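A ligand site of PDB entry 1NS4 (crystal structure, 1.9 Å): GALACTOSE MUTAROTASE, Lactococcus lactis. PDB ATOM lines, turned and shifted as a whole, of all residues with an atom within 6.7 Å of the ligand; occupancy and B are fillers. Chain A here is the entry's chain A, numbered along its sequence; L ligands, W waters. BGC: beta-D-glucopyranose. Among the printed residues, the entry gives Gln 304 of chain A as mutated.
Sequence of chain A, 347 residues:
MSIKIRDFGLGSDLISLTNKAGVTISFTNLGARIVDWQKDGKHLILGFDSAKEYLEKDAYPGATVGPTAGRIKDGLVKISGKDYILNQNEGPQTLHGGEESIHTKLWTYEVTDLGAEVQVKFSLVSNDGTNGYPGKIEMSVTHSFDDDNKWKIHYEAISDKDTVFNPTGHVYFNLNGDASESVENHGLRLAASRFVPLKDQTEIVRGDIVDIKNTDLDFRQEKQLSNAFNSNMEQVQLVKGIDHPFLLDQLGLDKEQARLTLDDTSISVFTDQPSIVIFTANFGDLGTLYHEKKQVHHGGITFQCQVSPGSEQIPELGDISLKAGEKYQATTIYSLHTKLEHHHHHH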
ATOM      1  N   ASP A  58      -7.772  -3.820  -6.266  1.00  0.00           N
ATOM      2  CA  ASP A  58      -7.737  -3.652  -7.710  1.00  0.00           C
ATOM      3  C   ASP A  58      -7.147  -2.293  -7.958  1.00  0.00           C
ATOM      4  O   ASP A  58      -7.742  -1.311  -7.498  1.00  0.00           O
ATOM      5  CB  ASP A  58      -9.149  -3.767  -8.332  1.00  0.00           C
ATOM      6  CG  ASP A  58      -9.111  -3.641  -9.827  1.00  0.00           C
ATOM      7  OD1 ASP A  58      -8.098  -3.384 -10.447  1.00  0.00           O
ATOM      8  OD2 ASP A  58     -10.270  -3.869 -10.407  1.00  0.00           O
ATOM      9  N   TYR A  60      -6.769  -0.675 -10.791  1.00  0.00           N
ATOM     10  CA  TYR A  60      -7.232   0.018 -11.973  1.00  0.00           C
ATOM     11  C   TYR A  60      -8.324   1.040 -11.857  1.00  0.00           C
ATOM     12  O   TYR A  60      -8.293   2.069 -12.580  1.00  0.00           O
ATOM     13  CB  TYR A  60      -7.613  -1.000 -13.056  1.00  0.00           C
ATOM     14  CG  TYR A  60      -6.385  -1.704 -13.588  1.00  0.00           C
ATOM     15  CD1 TYR A  60      -6.299  -3.097 -13.532  1.00  0.00           C
ATOM     16  CD2 TYR A  60      -5.310  -1.015 -14.158  1.00  0.00           C
ATOM     17  CE1 TYR A  60      -5.194  -3.789 -14.023  1.00  0.00           C
ATOM     18  CE2 TYR A  60      -4.189  -1.673 -14.645  1.00  0.00           C
ATOM     19  CZ  TYR A  60      -4.135  -3.066 -14.591  1.00  0.00           C
ATOM     20  OH  TYR A  60      -3.048  -3.728 -15.089  1.00  0.00           O
ATOM     21  N   PRO A  61      -9.316   0.772 -11.003  1.00  0.00           N
ATOM     22  CA  PRO A  61     -10.467   1.685 -10.892  1.00  0.00           C
ATOM     23  C   PRO A  61     -10.117   3.154 -10.724  1.00  0.00           C
ATOM     24  O   PRO A  61      -9.417   3.529  -9.793  1.00  0.00           O
ATOM     25  CB  PRO A  61     -11.342   1.145  -9.770  1.00  0.00           C
ATOM     26  CG  PRO A  61     -10.937  -0.314  -9.632  1.00  0.00           C
ATOM     27  CD  PRO A  61      -9.531  -0.451 -10.192  1.00  0.00           C
ATOM     28  N   GLY A  70      -5.074  -0.971 -22.613  1.00  0.00           N
ATOM     29  CA  GLY A  70      -5.584  -2.144 -23.304  1.00  0.00           C
ATOM     30  C   GLY A  70      -4.557  -3.224 -23.489  1.00  0.00           C
ATOM     31  O   GLY A  70      -3.468  -3.157 -22.935  1.00  0.00           O
ATOM     32  N   ARG A  71      -4.932  -4.246 -24.270  1.00  0.00           N
ATOM     33  CA  ARG A  71      -4.036  -5.330 -24.529  1.00  0.00           C
ATOM     34  C   ARG A  71      -3.324  -5.227 -25.827  1.00  0.00           C
ATOM     35  O   ARG A  71      -3.945  -4.925 -26.870  1.00  0.00           O
ATOM     36  CB  ARG A  71      -4.799  -6.643 -24.653  1.00  0.00           C
ATOM     37  CG  ARG A  71      -5.572  -6.942 -23.413  1.00  0.00           C
ATOM     38  CD  ARG A  71      -6.300  -8.296 -23.452  1.00  0.00           C
ATOM     39  NE  ARG A  71      -6.718  -8.575 -22.077  1.00  0.00           N
ATOM     40  CZ  ARG A  71      -7.788  -8.067 -21.453  1.00  0.00           C
ATOM     41  NH1 ARG A  71      -8.701  -7.258 -22.050  1.00  0.00           N
ATOM     42  NH2 ARG A  71      -7.943  -8.444 -20.179  1.00  0.00           N
ATOM     43  N   GLU A  90       0.021 -10.348 -18.637  1.00  0.00           N
ATOM     44  CA  GLU A  90      -1.207 -11.085 -18.709  1.00  0.00           C
ATOM     45  C   GLU A  90      -0.935 -12.153 -19.712  1.00  0.00           C
ATOM     46  O   GLU A  90      -1.217 -12.004 -20.901  1.00  0.00           O
ATOM     47  CB  GLU A  90      -2.336 -10.203 -19.207  1.00  0.00           C
ATOM     48  CG  GLU A  90      -3.629 -10.955 -18.962  1.00  0.00           C
ATOM     49  CD  GLU A  90      -4.765 -10.327 -19.700  1.00  0.00           C
ATOM     50  OE1 GLU A  90      -4.692 -10.043 -20.868  1.00  0.00           O
ATOM     51  OE2 GLU A  90      -5.841 -10.119 -18.963  1.00  0.00           O
ATOM     52  N   LEU A  95      -0.890  -5.800 -20.852  1.00  0.00           N
ATOM     53  CA  LEU A  95      -2.182  -5.195 -20.585  1.00  0.00           C
ATOM     54  C   LEU A  95      -1.965  -3.929 -19.781  1.00  0.00           C
ATOM     55  O   LEU A  95      -1.257  -3.956 -18.798  1.00  0.00           O
ATOM     56  CB  LEU A  95      -3.046  -6.139 -19.747  1.00  0.00           C
ATOM     57  CG  LEU A  95      -4.260  -5.443 -19.104  1.00  0.00           C
ATOM     58  CD1 LEU A  95      -5.409  -5.284 -20.104  1.00  0.00           C
ATOM     59  CD2 LEU A  95      -4.783  -6.295 -17.965  1.00  0.00           C
ATOM     60  N   HIS A  96      -2.567  -2.819 -20.200  1.00  0.00           N
ATOM     61  CA  HIS A  96      -2.419  -1.551 -19.477  1.00  0.00           C
ATOM     62  C   HIS A  96      -0.979  -1.136 -19.144  1.00  0.00           C
ATOM     63  O   HIS A  96      -0.701  -0.650 -18.047  1.00  0.00           O
ATOM     64  CB  HIS A  96      -3.295  -1.518 -18.210  1.00  0.00           C
ATOM     65  CG  HIS A  96      -4.756  -1.640 -18.546  1.00  0.00           C
ATOM     66  ND1 HIS A  96      -5.256  -1.197 -19.783  1.00  0.00           N
ATOM     67  CD2 HIS A  96      -5.778  -2.128 -17.828  1.00  0.00           C
ATOM     68  CE1 HIS A  96      -6.562  -1.441 -19.777  1.00  0.00           C
ATOM     69  NE2 HIS A  96      -6.914  -1.990 -18.622  1.00  0.00           N
ATOM     70  N   HIS A 170      -9.653   5.061 -16.431  1.00  0.00           N
ATOM     71  CA  HIS A 170     -10.371   3.850 -16.107  1.00  0.00           C
ATOM     72  C   HIS A 170     -11.477   3.936 -15.019  1.00  0.00           C
ATOM     73  O   HIS A 170     -11.696   3.000 -14.224  1.00  0.00           O
ATOM     74  CB  HIS A 170      -9.322   2.748 -15.776  1.00  0.00           C
ATOM     75  CG  HIS A 170      -9.732   1.323 -16.101  1.00  0.00           C
ATOM     76  ND1 HIS A 170     -10.703   0.641 -15.351  1.00  0.00           N
ATOM     77  CD2 HIS A 170      -9.295   0.482 -17.066  1.00  0.00           C
ATOM     78  CE1 HIS A 170     -10.834  -0.575 -15.898  1.00  0.00           C
ATOM     79  NE2 HIS A 170     -10.002  -0.703 -16.934  1.00  0.00           N
ATOM     80  N   TYR A 172     -15.042   3.601 -13.333  1.00  0.00           N
ATOM     81  CA  TYR A 172     -16.196   2.715 -13.442  1.00  0.00           C
ATOM     82  C   TYR A 172     -17.381   3.495 -12.853  1.00  0.00           C
ATOM     83  O   TYR A 172     -17.339   4.006 -11.721  1.00  0.00           O
ATOM     84  CB  TYR A 172     -16.098   1.489 -12.529  1.00  0.00           C
ATOM     85  CG  TYR A 172     -15.194   0.369 -12.999  1.00  0.00           C
ATOM     86  CD1 TYR A 172     -13.880   0.285 -12.547  1.00  0.00           C
ATOM     87  CD2 TYR A 172     -15.673  -0.648 -13.831  1.00  0.00           C
ATOM     88  CE1 TYR A 172     -13.041  -0.765 -12.937  1.00  0.00           C
ATOM     89  CE2 TYR A 172     -14.857  -1.694 -14.238  1.00  0.00           C
ATOM     90  CZ  TYR A 172     -13.540  -1.755 -13.785  1.00  0.00           C
ATOM     91  OH  TYR A 172     -12.725  -2.804 -14.147  1.00  0.00           O
ATOM     92  N   LEU A 198     -13.439  -9.776 -30.115  1.00  0.00           N
ATOM     93  CA  LEU A 198     -12.312 -10.405 -29.508  1.00  0.00           C
ATOM     94  C   LEU A 198     -12.126 -11.805 -30.048  1.00  0.00           C
ATOM     95  O   LEU A 198     -13.101 -12.483 -30.362  1.00  0.00           O
ATOM     96  CB  LEU A 198     -12.478 -10.458 -27.984  1.00  0.00           C
ATOM     97  CG  LEU A 198     -12.835  -9.078 -27.409  1.00  0.00           C
ATOM     98  CD1 LEU A 198     -12.894  -9.188 -25.881  1.00  0.00           C
ATOM     99  CD2 LEU A 198     -11.823  -7.991 -27.867  1.00  0.00           C
ATOM    100  N   GLU A 203      -8.775 -12.370 -25.059  1.00  0.00           N
ATOM    101  CA  GLU A 203      -9.213 -11.000 -25.285  1.00  0.00           C
ATOM    102  C   GLU A 203      -8.362 -10.213 -26.211  1.00  0.00           C
ATOM    103  O   GLU A 203      -8.416  -8.982 -26.210  1.00  0.00           O
ATOM    104  CB  GLU A 203      -9.570 -10.236 -24.009  1.00  0.00           C
ATOM    105  CG  GLU A 203     -10.742 -10.921 -23.234  1.00  0.00           C
ATOM    106  CD  GLU A 203     -11.008 -10.525 -21.788  1.00  0.00           C
ATOM    107  OE1 GLU A 203     -10.870 -11.271 -20.816  1.00  0.00           O
ATOM    108  OE2 GLU A 203     -11.502  -9.319 -21.662  1.00  0.00           O
ATOM    109  N   ASP A 243     -16.969  -6.082 -23.160  1.00  0.00           N
ATOM    110  CA  ASP A 243     -15.545  -5.855 -22.912  1.00  0.00           C
ATOM    111  C   ASP A 243     -14.967  -5.584 -24.264  1.00  0.00           C
ATOM    112  O   ASP A 243     -14.148  -6.337 -24.748  1.00  0.00           O
ATOM    113  CB  ASP A 243     -14.841  -7.049 -22.220  1.00  0.00           C
ATOM    114  CG  ASP A 243     -13.516  -6.635 -21.618  1.00  0.00           C
ATOM    115  OD1 ASP A 243     -13.074  -5.509 -21.738  1.00  0.00           O
ATOM    116  OD2 ASP A 243     -12.931  -7.559 -20.891  1.00  0.00           O
ATOM    117  N   HIS A 244     -15.438  -4.494 -24.868  1.00  0.00           N
ATOM    118  CA  HIS A 244     -15.044  -4.213 -26.216  1.00  0.00           C
ATOM    119  C   HIS A 244     -14.930  -2.774 -26.606  1.00  0.00           C
ATOM    120  O   HIS A 244     -15.627  -1.889 -26.077  1.00  0.00           O
ATOM    121  CB  HIS A 244     -16.242  -4.631 -27.121  1.00  0.00           C
ATOM    122  CG  HIS A 244     -16.454  -6.106 -27.135  1.00  0.00           C
ATOM    123  ND1 HIS A 244     -17.164  -6.756 -26.127  1.00  0.00           N
ATOM    124  CD2 HIS A 244     -16.049  -7.018 -28.062  1.00  0.00           C
ATOM    125  CE1 HIS A 244     -17.156  -8.056 -26.422  1.00  0.00           C
ATOM    126  NE2 HIS A 244     -16.505  -8.232 -27.588  1.00  0.00           N
ATOM    127  N   VAL A 277     -13.829   2.086 -25.107  1.00  0.00           N
ATOM    128  CA  VAL A 277     -13.815   0.729 -24.664  1.00  0.00           C
ATOM    129  C   VAL A 277     -14.792   0.564 -23.488  1.00  0.00           C
ATOM    130  O   VAL A 277     -14.631   1.191 -22.405  1.00  0.00           O
ATOM    131  CB  VAL A 277     -12.402   0.254 -24.304  1.00  0.00           C
ATOM    132  CG1 VAL A 277     -12.519  -1.186 -23.790  1.00  0.00           C
ATOM    133  CG2 VAL A 277     -11.486   0.309 -25.540  1.00  0.00           C
ATOM    134  N   ILE A 278     -15.775  -0.299 -23.679  1.00  0.00           N
ATOM    135  CA  ILE A 278     -16.785  -0.537 -22.653  1.00  0.00           C
ATOM    136  C   ILE A 278     -16.617  -1.893 -21.987  1.00  0.00           C
ATOM    137  O   ILE A 278     -16.689  -2.968 -22.631  1.00  0.00           O
ATOM    138  CB  ILE A 278     -18.196  -0.400 -23.245  1.00  0.00           C
ATOM    139  CG1 ILE A 278     -18.323   1.024 -23.772  1.00  0.00           C
ATOM    140  CG2 ILE A 278     -19.276  -0.683 -22.180  1.00  0.00           C
ATOM    141  CD1 ILE A 278     -19.694   1.347 -24.306  1.00  0.00           C
ATOM    142  N   PHE A 279     -16.394  -1.830 -20.689  1.00  0.00           N
ATOM    143  CA  PHE A 279     -16.195  -3.034 -19.893  1.00  0.00           C
ATOM    144  C   PHE A 279     -17.216  -2.990 -18.768  1.00  0.00           C
ATOM    145  O   PHE A 279     -17.270  -2.000 -18.029  1.00  0.00           O
ATOM    146  CB  PHE A 279     -14.718  -3.134 -19.436  1.00  0.00           C
ATOM    147  CG  PHE A 279     -14.438  -4.203 -18.416  1.00  0.00           C
ATOM    148  CD1 PHE A 279     -14.706  -5.537 -18.719  1.00  0.00           C
ATOM    149  CD2 PHE A 279     -13.958  -3.865 -17.160  1.00  0.00           C
ATOM    150  CE1 PHE A 279     -14.465  -6.537 -17.772  1.00  0.00           C
ATOM    151  CE2 PHE A 279     -13.728  -4.833 -16.190  1.00  0.00           C
ATOM    152  CZ  PHE A 279     -13.972  -6.170 -16.521  1.00  0.00           C
ATOM    153  N   PHE A 283     -16.889  -9.587 -13.449  1.00  0.00           N
ATOM    154  CA  PHE A 283     -16.072 -10.364 -12.480  1.00  0.00           C
ATOM    155  C   PHE A 283     -16.684 -11.572 -11.829  1.00  0.00           C
ATOM    156  O   PHE A 283     -16.087 -12.141 -10.905  1.00  0.00           O
ATOM    157  CB  PHE A 283     -15.438  -9.489 -11.377  1.00  0.00           C
ATOM    158  CG  PHE A 283     -14.697  -8.283 -11.918  1.00  0.00           C
ATOM    159  CD1 PHE A 283     -15.203  -6.987 -11.759  1.00  0.00           C
ATOM    160  CD2 PHE A 283     -13.488  -8.433 -12.606  1.00  0.00           C
ATOM    161  CE1 PHE A 283     -14.515  -5.866 -12.250  1.00  0.00           C
ATOM    162  CE2 PHE A 283     -12.785  -7.337 -13.103  1.00  0.00           C
ATOM    163  CZ  PHE A 283     -13.322  -6.049 -12.942  1.00  0.00           C
ATOM    164  N   THR A 302     -17.261   0.983 -17.660  1.00  0.00           N
ATOM    165  CA  THR A 302     -16.271   1.973 -18.016  1.00  0.00           C
ATOM    166  C   THR A 302     -16.598   2.602 -19.334  1.00  0.00           C
ATOM    167  O   THR A 302     -17.316   2.052 -20.143  1.00  0.00           O
ATOM    168  CB  THR A 302     -14.856   1.342 -18.230  1.00  0.00           C
ATOM    169  OG1 THR A 302     -14.928   0.558 -19.419  1.00  0.00           O
ATOM    170  CG2 THR A 302     -14.352   0.472 -17.076  1.00  0.00           C
ATOM    171  N   GLN A 304     -13.732   3.904 -21.554  1.00  0.00           N
ATOM    172  CA  GLN A 304     -12.316   4.205 -21.748  1.00  0.00           C
ATOM    173  C   GLN A 304     -12.138   4.814 -23.113  1.00  0.00           C
ATOM    174  O   GLN A 304     -12.217   4.121 -24.114  1.00  0.00           O
ATOM    175  CB  GLN A 304     -11.458   2.927 -21.647  1.00  0.00           C
ATOM    176  CG  GLN A 304     -11.653   2.266 -20.279  1.00  0.00           C
ATOM    177  CD  GLN A 304     -11.070   0.865 -20.216  1.00  0.00           C
ATOM    178  OE1 GLN A 304     -11.766  -0.130 -20.020  1.00  0.00           O
ATOM    179  NE2 GLN A 304      -9.769   0.787 -20.367  1.00  0.00           N
HETATM  180  C2  BGC L   1     -10.259  -4.694 -19.626  1.00  0.00           C
HETATM  181  C3  BGC L   1     -10.806  -5.971 -19.055  1.00  0.00           C
HETATM  182  C4  BGC L   1      -9.964  -6.356 -17.852  1.00  0.00           C
HETATM  183  C5  BGC L   1      -9.949  -5.185 -16.883  1.00  0.00           C
HETATM  184  C6  BGC L   1      -9.046  -5.388 -15.705  1.00  0.00           C
HETATM  185  C1  BGC L   1     -10.370  -3.608 -18.564  1.00  0.00           C
HETATM  186  O1  BGC L   1     -10.006  -2.328 -19.073  1.00  0.00           O
HETATM  187  O2  BGC L   1     -11.050  -4.396 -20.775  1.00  0.00           O
HETATM  188  O3  BGC L   1     -10.682  -6.992 -20.013  1.00  0.00           O
HETATM  189  O4  BGC L   1     -10.457  -7.528 -17.205  1.00  0.00           O
HETATM  190  O5  BGC L   1      -9.477  -3.956 -17.525  1.00  0.00           O
HETATM  191  O6  BGC L   1      -9.237  -4.250 -14.888  1.00  0.00           O
HETATM  192  O   HOH W   1     -10.491  -3.155 -12.719  1.00  0.00           O
HETATM  193  O   HOH W   2      -9.303  -3.242 -22.769  1.00  0.00           O
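O3 of the ligand is in hydrogen-bond range of OD2 of Asp 243 (2.5 Å).
NE2 of His 170 lies within hydrogen-bond range of O1 of the ligand, 2.7 Å away.
The guanidinium group of Arg 71 sits at hydrogen-bond distance from an oxygen (O3) of the ligand (2.9 Å).
OE2 of Glu 203 is in hydrogen-bond range of O3 of the ligand, 3.0 Å away.
The side-chain amide oxygen (OE1) of Gln 304 lies within hydrogen-bond range of an oxygen (O1) of the ligand (3.0 Å).
A ring nitrogen (NE2) of His 96 is in hydrogen-bond range of an oxygen (O1) of the ligand, 3.1 Å away.
The backbone NH of Asp 243 lies close to the backbone carbonyl oxygen of Ile 278 (3.2 Å).
The guanidinium group (NH1) of Arg 71 lies within salt-bridge range of the side-chain carboxylate (OE2) of Glu 203 (3.5 Å).
NE of Arg 71 is in salt-bridge range of OE1 of Glu 90 (2.8 Å).
O of Gln 304 is in hydrogen-bond range of N of Val 277 (2.8 Å).
OE1 of Gln 304 sits at hydrogen-bond distance from OG1 of Thr 302, at 3.3 Å.
ND1 of His 96 is in hydrogen-bond range of N of Gly 70 (2.8 Å).
N of Tyr 60 lies within hydrogen-bond range of OD1 of Asp 58 (3.0 Å).
The backbone carbonyl oxygen (O) of Phe 279 sits at hydrogen-bond distance from the backbone NH (N) of Thr 302 (3.0 Å).
Water W1 lies within hydrogen-bond range of OD2 of Asp 58 (2.4 Å), OH of Tyr 172 (2.7 Å) and O6 of the ligand (2.7 Å).
CD1 of Tyr 60 touches O6 of the ligand, at 3.4 Å.
Tyr 172 touches the ligand.
Phe 279 touches the ligand (CZ to O4, 3.8 Å).
Hydrophobic or aromatic side chains that line the ligand: Tyr 60, His 96, His 170 and Phe 279.
Nine residues have an atom within 4 Å of the ligand: Tyr 60, Arg 71, His 96, His 170, Tyr 172, Glu 203, Asp 243, Phe 279 and Gln 304.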
